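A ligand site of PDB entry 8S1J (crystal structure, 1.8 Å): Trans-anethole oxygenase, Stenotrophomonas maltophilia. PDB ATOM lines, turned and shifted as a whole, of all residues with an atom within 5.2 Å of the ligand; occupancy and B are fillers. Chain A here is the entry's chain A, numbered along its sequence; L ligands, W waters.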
ATOM      1  N   PHE A  51     -14.413  20.594 -29.955  1.00  0.00           N
ATOM      2  CA  PHE A  51     -13.013  20.700 -30.319  1.00  0.00           C
ATOM      3  C   PHE A  51     -12.328  19.329 -30.282  1.00  0.00           C
ATOM      4  O   PHE A  51     -11.324  19.130 -30.973  1.00  0.00           O
ATOM      5  CB  PHE A  51     -12.224  21.641 -29.404  1.00  0.00           C
ATOM      6  CG  PHE A  51     -12.835  23.032 -29.214  1.00  0.00           C
ATOM      7  CD1 PHE A  51     -13.737  23.553 -30.143  1.00  0.00           C
ATOM      8  CD2 PHE A  51     -12.511  23.812 -28.106  1.00  0.00           C
ATOM      9  CE1 PHE A  51     -14.325  24.793 -29.919  1.00  0.00           C
ATOM     10  CE2 PHE A  51     -13.087  25.043 -27.898  1.00  0.00           C
ATOM     11  CZ  PHE A  51     -14.000  25.523 -28.797  1.00  0.00           C
ATOM     12  N   THR A  52     -12.836  18.421 -29.443  1.00  0.00           N
ATOM     13  CA  THR A  52     -12.175  17.161 -29.184  1.00  0.00           C
ATOM     14  C   THR A  52     -12.921  16.000 -29.854  1.00  0.00           C
ATOM     15  O   THR A  52     -12.845  14.881 -29.376  1.00  0.00           O
ATOM     16  CB  THR A  52     -11.989  16.935 -27.681  1.00  0.00           C
ATOM     17  OG1 THR A  52     -13.244  17.018 -26.999  1.00  0.00           O
ATOM     18  CG2 THR A  52     -10.971  17.911 -27.096  1.00  0.00           C
ATOM     19  N   GLY A  57      -7.516  14.385 -29.349  1.00  0.00           N
ATOM     20  CA  GLY A  57      -7.804  15.523 -28.496  1.00  0.00           C
ATOM     21  C   GLY A  57      -8.479  15.130 -27.171  1.00  0.00           C
ATOM     22  O   GLY A  57      -8.125  15.639 -26.137  1.00  0.00           O
ATOM     23  N   MET A  60      -5.778  13.505 -25.146  1.00  0.00           N
ATOM     24  CA  MET A  60      -4.874  14.533 -24.641  1.00  0.00           C
ATOM     25  C   MET A  60      -5.447  15.228 -23.394  1.00  0.00           C
ATOM     26  O   MET A  60      -4.786  15.292 -22.348  1.00  0.00           O
ATOM     27  CB  MET A  60      -4.571  15.543 -25.750  1.00  0.00           C
ATOM     28  CG  MET A  60      -3.770  16.792 -25.370  1.00  0.00           C
ATOM     29  SD  MET A  60      -2.179  16.440 -24.608  1.00  0.00           S
ATOM     30  CE  MET A  60      -1.356  15.990 -26.146  1.00  0.00           C
ATOM     31  N   MET A  61      -6.678  15.708 -23.469  1.00  0.00           N
ATOM     32  CA  MET A  61      -7.240  16.462 -22.330  1.00  0.00           C
ATOM     33  C   MET A  61      -7.637  15.533 -21.182  1.00  0.00           C
ATOM     34  O   MET A  61      -7.358  15.814 -20.011  1.00  0.00           O
ATOM     35  CB  MET A  61      -8.461  17.270 -22.763  1.00  0.00           C
ATOM     36  CG  MET A  61      -8.148  18.350 -23.788  1.00  0.00           C
ATOM     37  SD  MET A  61      -9.499  19.531 -23.973  1.00  0.00           S
ATOM     38  CE  MET A  61      -8.838  20.665 -25.206  1.00  0.00           C
ATOM     39  N   THR A  65      -3.223  14.918 -19.848  1.00  0.00           N
ATOM     40  CA  THR A  65      -3.028  15.969 -18.862  1.00  0.00           C
ATOM     41  C   THR A  65      -4.039  15.840 -17.722  1.00  0.00           C
ATOM     42  O   THR A  65      -3.714  16.220 -16.606  1.00  0.00           O
ATOM     43  CB  THR A  65      -3.127  17.368 -19.467  1.00  0.00           C
ATOM     44  OG1 THR A  65      -4.523  17.650 -19.659  1.00  0.00           O
ATOM     45  CG2 THR A  65      -2.332  17.470 -20.754  1.00  0.00           C
ATOM     46  N   LYS A  67      -6.450  17.673 -16.949  1.00  0.00           N
ATOM     47  CA  LYS A  67      -6.770  18.931 -16.278  1.00  0.00           C
ATOM     48  C   LYS A  67      -8.275  19.156 -16.287  1.00  0.00           C
ATOM     49  O   LYS A  67      -8.816  19.589 -15.292  1.00  0.00           O
ATOM     50  CB  LYS A  67      -5.968  20.066 -16.936  1.00  0.00           C
ATOM     51  CG  LYS A  67      -6.189  21.432 -16.290  1.00  0.00           C
ATOM     52  CD  LYS A  67      -5.291  22.576 -16.781  1.00  0.00           C
ATOM     53  CE  LYS A  67      -5.572  23.834 -16.014  1.00  0.00           C
ATOM     54  NZ  LYS A  67      -4.909  25.041 -16.516  1.00  0.00           N
ATOM     55  N   ALA A  68      -8.962  18.862 -17.401  1.00  0.00           N
ATOM     56  CA  ALA A  68     -10.407  18.975 -17.502  1.00  0.00           C
ATOM     57  C   ALA A  68     -11.126  18.020 -16.561  1.00  0.00           C
ATOM     58  O   ALA A  68     -12.224  18.340 -16.103  1.00  0.00           O
ATOM     59  CB  ALA A  68     -10.856  18.735 -18.925  1.00  0.00           C
ATOM     60  N   ARG A  75      -9.492  24.810 -15.376  1.00  0.00           N
ATOM     61  CA  ARG A  75      -9.334  24.751 -16.815  1.00  0.00           C
ATOM     62  C   ARG A  75     -10.264  25.773 -17.479  1.00  0.00           C
ATOM     63  O   ARG A  75      -9.844  26.513 -18.386  1.00  0.00           O
ATOM     64  CB  ARG A  75      -9.552  23.293 -17.221  1.00  0.00           C
ATOM     65  CG  ARG A  75      -9.488  22.855 -18.678  1.00  0.00           C
ATOM     66  CD  ARG A  75      -8.608  23.607 -19.613  1.00  0.00           C
ATOM     67  NE  ARG A  75      -8.287  22.796 -20.805  1.00  0.00           N
ATOM     68  CZ  ARG A  75      -8.431  23.203 -22.071  1.00  0.00           C
ATOM     69  NH1 ARG A  75      -9.362  24.057 -22.400  1.00  0.00           N
ATOM     70  NH2 ARG A  75      -7.667  22.686 -23.026  1.00  0.00           N
ATOM     71  N   ASP A  78      -9.016  29.257 -16.662  1.00  0.00           N
ATOM     72  CA  ASP A  78      -7.756  29.504 -17.360  1.00  0.00           C
ATOM     73  C   ASP A  78      -7.976  29.761 -18.852  1.00  0.00           C
ATOM     74  O   ASP A  78      -7.338  30.668 -19.406  1.00  0.00           O
ATOM     75  CB  ASP A  78      -6.752  28.389 -17.109  1.00  0.00           C
ATOM     76  CG  ASP A  78      -6.222  28.346 -15.679  1.00  0.00           C
ATOM     77  OD1 ASP A  78      -6.567  29.246 -14.919  1.00  0.00           O
ATOM     78  OD2 ASP A  78      -5.514  27.396 -15.362  1.00  0.00           O
ATOM     79  N   THR A  79      -8.841  28.962 -19.496  1.00  0.00           N
ATOM     80  CA  THR A  79      -9.153  29.161 -20.907  1.00  0.00           C
ATOM     81  C   THR A  79      -9.792  30.520 -21.112  1.00  0.00           C
ATOM     82  O   THR A  79      -9.422  31.270 -22.022  1.00  0.00           O
ATOM     83  CB  THR A  79     -10.099  28.074 -21.407  1.00  0.00           C
ATOM     84  OG1 THR A  79      -9.437  26.834 -21.211  1.00  0.00           O
ATOM     85  CG2 THR A  79     -10.425  28.242 -22.880  1.00  0.00           C
ATOM     86  N   HIS A  82      -7.880  33.909 -21.248  1.00  0.00           N
ATOM     87  CA  HIS A  82      -7.335  34.155 -22.574  1.00  0.00           C
ATOM     88  C   HIS A  82      -8.444  34.658 -23.501  1.00  0.00           C
ATOM     89  O   HIS A  82      -8.289  35.653 -24.203  1.00  0.00           O
ATOM     90  CB  HIS A  82      -6.646  32.891 -23.113  1.00  0.00           C
ATOM     91  CG  HIS A  82      -5.370  32.473 -22.424  1.00  0.00           C
ATOM     92  ND1 HIS A  82      -4.170  33.123 -22.612  1.00  0.00           N
ATOM     93  CD2 HIS A  82      -5.120  31.503 -21.538  1.00  0.00           C
ATOM     94  CE1 HIS A  82      -3.222  32.521 -21.901  1.00  0.00           C
ATOM     95  NE2 HIS A  82      -3.785  31.533 -21.234  1.00  0.00           N
ATOM     96  N   PHE A  83      -9.603  33.987 -23.524  1.00  0.00           N
ATOM     97  CA  PHE A  83     -10.615  34.299 -24.526  1.00  0.00           C
ATOM     98  C   PHE A  83     -11.126  35.728 -24.333  1.00  0.00           C
ATOM     99  O   PHE A  83     -11.231  36.496 -25.305  1.00  0.00           O
ATOM    100  CB  PHE A  83     -11.805  33.338 -24.531  1.00  0.00           C
ATOM    101  CG  PHE A  83     -11.626  31.922 -25.094  1.00  0.00           C
ATOM    102  CD1 PHE A  83     -10.393  31.450 -25.531  1.00  0.00           C
ATOM    103  CD2 PHE A  83     -12.731  31.080 -25.186  1.00  0.00           C
ATOM    104  CE1 PHE A  83     -10.275  30.156 -26.016  1.00  0.00           C
ATOM    105  CE2 PHE A  83     -12.606  29.785 -25.680  1.00  0.00           C
ATOM    106  CZ  PHE A  83     -11.377  29.324 -26.081  1.00  0.00           C
ATOM    107  N   TRP A  86      -8.503  38.170 -25.652  1.00  0.00           N
ATOM    108  CA  TRP A  86      -8.538  38.234 -27.121  1.00  0.00           C
ATOM    109  C   TRP A  86      -9.751  39.022 -27.611  1.00  0.00           C
ATOM    110  O   TRP A  86      -9.670  39.807 -28.561  1.00  0.00           O
ATOM    111  CB  TRP A  86      -8.547  36.861 -27.785  1.00  0.00           C
ATOM    112  CG  TRP A  86      -7.447  35.925 -27.395  1.00  0.00           C
ATOM    113  CD1 TRP A  86      -6.300  36.210 -26.694  1.00  0.00           C
ATOM    114  CD2 TRP A  86      -7.419  34.504 -27.643  1.00  0.00           C
ATOM    115  NE1 TRP A  86      -5.566  35.069 -26.507  1.00  0.00           N
ATOM    116  CE2 TRP A  86      -6.228  34.007 -27.073  1.00  0.00           C
ATOM    117  CE3 TRP A  86      -8.291  33.605 -28.280  1.00  0.00           C
ATOM    118  CZ2 TRP A  86      -5.904  32.661 -27.097  1.00  0.00           C
ATOM    119  CZ3 TRP A  86      -7.980  32.269 -28.288  1.00  0.00           C
ATOM    120  CH2 TRP A  86      -6.795  31.803 -27.710  1.00  0.00           C
ATOM    121  N   VAL A 103      -0.376  30.460 -25.288  1.00  0.00           N
ATOM    122  CA  VAL A 103      -1.174  29.321 -25.718  1.00  0.00           C
ATOM    123  C   VAL A 103      -0.412  28.544 -26.786  1.00  0.00           C
ATOM    124  O   VAL A 103      -0.318  27.322 -26.715  1.00  0.00           O
ATOM    125  CB  VAL A 103      -2.583  29.771 -26.194  1.00  0.00           C
ATOM    126  CG1 VAL A 103      -3.419  28.602 -26.706  1.00  0.00           C
ATOM    127  CG2 VAL A 103      -3.348  30.469 -25.075  1.00  0.00           C
ATOM    128  N   ILE A 106       2.156  26.450 -25.065  1.00  0.00           N
ATOM    129  CA  ILE A 106       1.524  25.312 -24.411  1.00  0.00           C
ATOM    130  C   ILE A 106       1.247  24.222 -25.438  1.00  0.00           C
ATOM    131  O   ILE A 106       1.578  23.058 -25.215  1.00  0.00           O
ATOM    132  CB  ILE A 106       0.229  25.717 -23.690  1.00  0.00           C
ATOM    133  CG1 ILE A 106       0.536  26.637 -22.495  1.00  0.00           C
ATOM    134  CG2 ILE A 106      -0.557  24.481 -23.261  1.00  0.00           C
ATOM    135  CD1 ILE A 106      -0.663  27.419 -21.985  1.00  0.00           C
ATOM    136  N   HIS A 107       0.599  24.588 -26.557  1.00  0.00           N
ATOM    137  CA  HIS A 107       0.240  23.599 -27.561  1.00  0.00           C
ATOM    138  C   HIS A 107       1.497  22.926 -28.143  1.00  0.00           C
ATOM    139  O   HIS A 107       1.502  21.724 -28.439  1.00  0.00           O
ATOM    140  CB  HIS A 107      -0.581  24.247 -28.684  1.00  0.00           C
ATOM    141  CG  HIS A 107      -1.984  24.622 -28.293  1.00  0.00           C
ATOM    142  ND1 HIS A 107      -2.690  25.590 -28.995  1.00  0.00           N
ATOM    143  CD2 HIS A 107      -2.825  24.190 -27.319  1.00  0.00           C
ATOM    144  CE1 HIS A 107      -3.890  25.712 -28.461  1.00  0.00           C
ATOM    145  NE2 HIS A 107      -3.987  24.878 -27.445  1.00  0.00           N
ATOM    146  N   LEU A 110       2.653  20.207 -25.827  1.00  0.00           N
ATOM    147  CA  LEU A 110       1.703  19.112 -25.893  1.00  0.00           C
ATOM    148  C   LEU A 110       1.889  18.293 -27.155  1.00  0.00           C
ATOM    149  O   LEU A 110       1.755  17.066 -27.088  1.00  0.00           O
ATOM    150  CB  LEU A 110       0.295  19.685 -25.779  1.00  0.00           C
ATOM    151  CG  LEU A 110      -0.014  20.396 -24.460  1.00  0.00           C
ATOM    152  CD1 LEU A 110      -1.397  20.979 -24.456  1.00  0.00           C
ATOM    153  CD2 LEU A 110       0.157  19.419 -23.317  1.00  0.00           C
ATOM    154  N   THR A 117      -1.870  15.809 -32.697  1.00  0.00           N
ATOM    155  CA  THR A 117      -2.964  16.370 -31.906  1.00  0.00           C
ATOM    156  C   THR A 117      -3.347  17.785 -32.381  1.00  0.00           C
ATOM    157  O   THR A 117      -4.463  18.264 -32.120  1.00  0.00           O
ATOM    158  CB  THR A 117      -2.550  16.320 -30.428  1.00  0.00           C
ATOM    159  OG1 THR A 117      -2.331  14.958 -30.100  1.00  0.00           O
ATOM    160  CG2 THR A 117      -3.612  16.812 -29.469  1.00  0.00           C
ATOM    161  N   PHE A 118      -2.449  18.497 -33.069  1.00  0.00           N
ATOM    162  CA  PHE A 118      -2.676  19.889 -33.418  1.00  0.00           C
ATOM    163  C   PHE A 118      -2.506  20.140 -34.917  1.00  0.00           C
ATOM    164  O   PHE A 118      -1.731  21.016 -35.322  1.00  0.00           O
ATOM    165  CB  PHE A 118      -1.745  20.758 -32.568  1.00  0.00           C
ATOM    166  CG  PHE A 118      -2.013  20.699 -31.074  1.00  0.00           C
ATOM    167  CD1 PHE A 118      -2.989  21.518 -30.488  1.00  0.00           C
ATOM    168  CD2 PHE A 118      -1.313  19.832 -30.251  1.00  0.00           C
ATOM    169  CE1 PHE A 118      -3.244  21.448 -29.137  1.00  0.00           C
ATOM    170  CE2 PHE A 118      -1.582  19.762 -28.899  1.00  0.00           C
ATOM    171  CZ  PHE A 118      -2.525  20.590 -28.337  1.00  0.00           C
ATOM    172  N   ASP A 122      -7.655  21.413 -37.162  1.00  0.00           N
ATOM    173  CA  ASP A 122      -8.340  21.520 -35.880  1.00  0.00           C
ATOM    174  C   ASP A 122      -8.249  22.941 -35.317  1.00  0.00           C
ATOM    175  O   ASP A 122      -9.146  23.399 -34.596  1.00  0.00           O
ATOM    176  CB  ASP A 122      -7.861  20.477 -34.897  1.00  0.00           C
ATOM    177  CG  ASP A 122      -8.217  19.060 -35.275  1.00  0.00           C
ATOM    178  OD1 ASP A 122      -9.205  18.893 -36.043  1.00  0.00           O
ATOM    179  OD2 ASP A 122      -7.487  18.141 -34.824  1.00  0.00           O
ATOM    180  N   VAL A 123      -7.173  23.643 -35.669  1.00  0.00           N
ATOM    181  CA  VAL A 123      -7.091  25.053 -35.319  1.00  0.00           C
ATOM    182  C   VAL A 123      -8.158  25.827 -36.103  1.00  0.00           C
ATOM    183  O   VAL A 123      -8.856  26.621 -35.511  1.00  0.00           O
ATOM    184  CB  VAL A 123      -5.677  25.599 -35.487  1.00  0.00           C
ATOM    185  CG1 VAL A 123      -5.632  27.110 -35.233  1.00  0.00           C
ATOM    186  CG2 VAL A 123      -4.713  24.868 -34.543  1.00  0.00           C
ATOM    187  N   THR A 126     -11.646  24.830 -34.517  1.00  0.00           N
ATOM    188  CA  THR A 126     -11.907  25.320 -33.182  1.00  0.00           C
ATOM    189  C   THR A 126     -12.131  26.824 -33.247  1.00  0.00           C
ATOM    190  O   THR A 126     -13.066  27.341 -32.636  1.00  0.00           O
ATOM    191  CB  THR A 126     -10.740  24.975 -32.260  1.00  0.00           C
ATOM    192  OG1 THR A 126     -10.786  23.577 -32.017  1.00  0.00           O
ATOM    193  CG2 THR A 126     -10.895  25.634 -30.894  1.00  0.00           C
ATOM    194  N   SER A 127     -11.273  27.537 -33.981  1.00  0.00           N
ATOM    195  CA  SER A 127     -11.457  28.959 -34.065  1.00  0.00           C
ATOM    196  C   SER A 127     -12.768  29.267 -34.792  1.00  0.00           C
ATOM    197  O   SER A 127     -13.508  30.171 -34.402  1.00  0.00           O
ATOM    198  CB  SER A 127     -10.289  29.628 -34.675  1.00  0.00           C
ATOM    199  OG  SER A 127     -10.037  29.118 -35.967  1.00  0.00           O
ATOM    200  N   ILE A 130     -15.739  28.925 -32.595  1.00  0.00           N
ATOM    201  CA  ILE A 130     -15.903  29.992 -31.641  1.00  0.00           C
ATOM    202  C   ILE A 130     -16.491  31.219 -32.342  1.00  0.00           C
ATOM    203  O   ILE A 130     -17.360  31.885 -31.796  1.00  0.00           O
ATOM    204  CB  ILE A 130     -14.575  30.344 -30.924  1.00  0.00           C
ATOM    205  CG1 ILE A 130     -14.041  29.179 -30.139  1.00  0.00           C
ATOM    206  CG2 ILE A 130     -14.793  31.581 -30.030  1.00  0.00           C
ATOM    207  CD1 ILE A 130     -12.670  29.389 -29.526  1.00  0.00           C
ATOM    208  N   TRP A 158     -11.374  36.307 -36.746  1.00  0.00           N
ATOM    209  CA  TRP A 158     -10.872  34.949 -36.626  1.00  0.00           C
ATOM    210  C   TRP A 158      -9.872  34.608 -37.728  1.00  0.00           C
ATOM    211  O   TRP A 158      -8.926  33.844 -37.479  1.00  0.00           O
ATOM    212  CB  TRP A 158     -12.015  33.928 -36.514  1.00  0.00           C
ATOM    213  CG  TRP A 158     -12.591  34.004 -35.130  1.00  0.00           C
ATOM    214  CD1 TRP A 158     -13.740  34.604 -34.731  1.00  0.00           C
ATOM    215  CD2 TRP A 158     -11.870  33.627 -33.926  1.00  0.00           C
ATOM    216  NE1 TRP A 158     -13.828  34.562 -33.363  1.00  0.00           N
ATOM    217  CE2 TRP A 158     -12.687  34.005 -32.844  1.00  0.00           C
ATOM    218  CE3 TRP A 158     -10.644  33.019 -33.672  1.00  0.00           C
ATOM    219  CZ2 TRP A 158     -12.308  33.765 -31.533  1.00  0.00           C
ATOM    220  CZ3 TRP A 158     -10.259  32.798 -32.369  1.00  0.00           C
ATOM    221  CH2 TRP A 158     -11.078  33.196 -31.315  1.00  0.00           C
ATOM    222  N   PHE A 165      -1.895  31.881 -35.220  1.00  0.00           N
ATOM    223  CA  PHE A 165      -2.177  30.699 -34.412  1.00  0.00           C
ATOM    224  C   PHE A 165      -1.309  29.542 -34.900  1.00  0.00           C
ATOM    225  O   PHE A 165      -1.356  29.188 -36.074  1.00  0.00           O
ATOM    226  CB  PHE A 165      -3.661  30.352 -34.536  1.00  0.00           C
ATOM    227  CG  PHE A 165      -4.281  29.918 -33.216  1.00  0.00           C
ATOM    228  CD1 PHE A 165      -3.886  28.734 -32.608  1.00  0.00           C
ATOM    229  CD2 PHE A 165      -5.231  30.696 -32.583  1.00  0.00           C
ATOM    230  CE1 PHE A 165      -4.425  28.328 -31.404  1.00  0.00           C
ATOM    231  CE2 PHE A 165      -5.784  30.290 -31.378  1.00  0.00           C
ATOM    232  CZ  PHE A 165      -5.371  29.116 -30.793  1.00  0.00           C
HETATM  233  C1  LIG L   1      -4.607  25.026 -23.375  1.00  0.00           C
HETATM  234  C2  LIG L   1      -5.608  21.070 -25.924  1.00  0.00           C
HETATM  235  C3  LIG L   1      -6.818  23.873 -29.749  1.00  0.00           C
HETATM  236  C4  LIG L   1      -7.158  27.543 -26.593  1.00  0.00           C
HETATM  237  C5  LIG L   1      -4.681  23.715 -23.797  1.00  0.00           C
HETATM  238  C6  LIG L   1      -4.288  22.612 -23.012  1.00  0.00           C
HETATM  239  C7  LIG L   1      -4.569  21.513 -23.733  1.00  0.00           C
HETATM  240  C8  LIG L   1      -5.167  21.918 -24.928  1.00  0.00           C
HETATM  241  C9  LIG L   1      -4.329  20.071 -23.335  1.00  0.00           C
HETATM  242  C10 LIG L   1      -3.600  22.657 -21.649  1.00  0.00           C
HETATM  243  C11 LIG L   1      -4.578  22.568 -20.470  1.00  0.00           C
HETATM  244  C12 LIG L   1      -5.011  21.115 -20.306  1.00  0.00           C
HETATM  245  O1  LIG L   1      -4.172  20.254 -19.910  1.00  0.00           O
HETATM  246  O2  LIG L   1      -6.192  20.783 -20.584  1.00  0.00           O
HETATM  247  C13 LIG L   1      -6.035  21.511 -27.188  1.00  0.00           C
HETATM  248  C14 LIG L   1      -6.289  20.591 -28.225  1.00  0.00           C
HETATM  249  C15 LIG L   1      -6.581  21.341 -29.333  1.00  0.00           C
HETATM  250  C16 LIG L   1      -6.528  22.772 -28.930  1.00  0.00           C
HETATM  251  C17 LIG L   1      -6.216  19.070 -28.165  1.00  0.00           C
HETATM  252  C18 LIG L   1      -7.025  20.752 -30.593  1.00  0.00           C
HETATM  253  C19 LIG L   1      -7.913  21.363 -31.345  1.00  0.00           C
HETATM  254  C20 LIG L   1      -7.062  25.129 -29.235  1.00  0.00           C
HETATM  255  C21 LIG L   1      -7.579  26.255 -29.915  1.00  0.00           C
HETATM  256  C22 LIG L   1      -7.699  27.281 -29.002  1.00  0.00           C
HETATM  257  C23 LIG L   1      -7.258  26.779 -27.739  1.00  0.00           C
HETATM  258  C24 LIG L   1      -7.939  26.354 -31.363  1.00  0.00           C
HETATM  259  C25 LIG L   1      -8.204  28.648 -29.214  1.00  0.00           C
HETATM  260  C26 LIG L   1      -8.749  29.142 -30.331  1.00  0.00           C
HETATM  261  C27 LIG L   1      -6.447  27.137 -25.473  1.00  0.00           C
HETATM  262  C28 LIG L   1      -6.229  28.038 -24.311  1.00  0.00           C
HETATM  263  C29 LIG L   1      -5.518  27.331 -23.405  1.00  0.00           C
HETATM  264  C30 LIG L   1      -5.294  26.024 -24.037  1.00  0.00           C
HETATM  265  C31 LIG L   1      -6.697  29.487 -24.187  1.00  0.00           C
HETATM  266  C32 LIG L   1      -5.043  27.769 -22.027  1.00  0.00           C
HETATM  267  C33 LIG L   1      -5.913  27.018 -20.943  1.00  0.00           C
HETATM  268  C34 LIG L   1      -5.138  26.491 -19.731  1.00  0.00           C
HETATM  269  O3  LIG L   1      -4.059  27.095 -19.450  1.00  0.00           O
HETATM  270  O4  LIG L   1      -5.520  25.470 -19.033  1.00  0.00           O
HETATM  271  N1  LIG L   1      -5.242  23.249 -24.973  1.00  0.00           N
HETATM  272  N2  LIG L   1      -6.183  22.752 -27.637  1.00  0.00           N
HETATM  273  N3  LIG L   1      -6.890  25.482 -27.946  1.00  0.00           N
HETATM  274  N4  LIG L   1      -5.877  25.948 -25.275  1.00  0.00           N
HETATM  275 FE1  LIG L   1      -5.886  24.443 -26.451  1.00  0.00          FE
HETATM  276  O   HOH W   1      -7.631  18.770 -19.769  1.00  0.00           O
HETATM  277  O   HOH W   2      -1.971  20.782 -18.967  1.00  0.00           O
HETATM  278  O   HOH W   3      -8.706  24.482 -25.629  1.00  0.00           O
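An iron atom (FE1) of the ligand is bound by a ring nitrogen (NE2) of His 107 (2.2 Å).
An oxygen (O4) of the ligand is in salt-bridge range of the side-chain amino group (NZ) of Lys 67, 2.6 Å away.
OG1 of Thr 65 sits at hydrogen-bond distance from O1 of the ligand.
The guanidinium group (NE) of Arg 75 is in salt-bridge range of an oxygen (O2) of the ligand.
N of Lys 67 sits close to OG1 of Thr 65 (3.3 Å).
The side-chain amino group of Lys 67 lies within salt-bridge range of the side-chain carboxylate of Asp 78 (2.7 Å).
The backbone carbonyl oxygen (O) of Met 61 is in hydrogen-bond range of the side-chain hydroxyl (OG1) of Thr 65, at 3.4 Å.
The backbone NH (N) of Thr 65 lies within hydrogen-bond range of the backbone carbonyl oxygen (O) of Met 60 (3.0 Å).
The guanidinium group (NH2) of Arg 75 sits close to the side-chain sulfur (SD) of Met 61, at 3.8 Å.
The side-chain hydroxyl of Thr 79 sits at hydrogen-bond distance from the backbone carbonyl oxygen of Arg 75, at 2.9 Å.
The side-chain hydroxyl (OG1) of Thr 126 lies within hydrogen-bond range of the backbone carbonyl oxygen (O) of Asp 122 (3.1 Å).
Gly 57 touches the ligand (CA to C17, 3.9 Å).
Met 60 touches the ligand (CG to C9, 3.9 Å).
CE of Met 61 touches C2 of the ligand (3.3 Å).
Asp 78 touches the ligand (CB to C34, 3.6 Å).
Thr 79 touches the ligand (OG1 to C33, 3.5 Å).
His 82 touches the ligand.
Trp 86 touches the ligand (CZ3 to C25, 3.7 Å).
CG1 of Val 103 touches C27 of the ligand, at 3.6 Å.
Ile 106 touches the ligand (CG2 to C10, 3.9 Å).
Leu 110 touches the ligand (CD1 to C9, 3.3 Å).
CG2 of Thr 117 touches C17 of the ligand (3.7 Å).
Phe 118 touches the ligand.
Asp 122 touches the ligand (CB to C19, 3.7 Å).
Thr 126 touches the ligand (CG2 to C24, 3.1 Å).
Phe 165 touches the ligand.
Hydrophobic or aromatic side chains that line the ligand: Met 60, Met 61, His 82, Trp 86, Val 103, Ile 106, His 107, Leu 110, Phe 118 and Phe 165.
The nearest printed residue that does not touch the ligand is Ile 130 (4.01 Å).
Water W1 lies within hydrogen-bond range of an oxygen (O2) of the ligand (2.6 Å), the backbone NH (N) of Ala 68 (2.7 Å), the backbone carbonyl oxygen (O) of Met 61 (3.0 Å), the backbone NH (N) of Lys 67 (3.2 Å) and the side-chain hydroxyl (OG1) of Thr 65 (3.3 Å).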
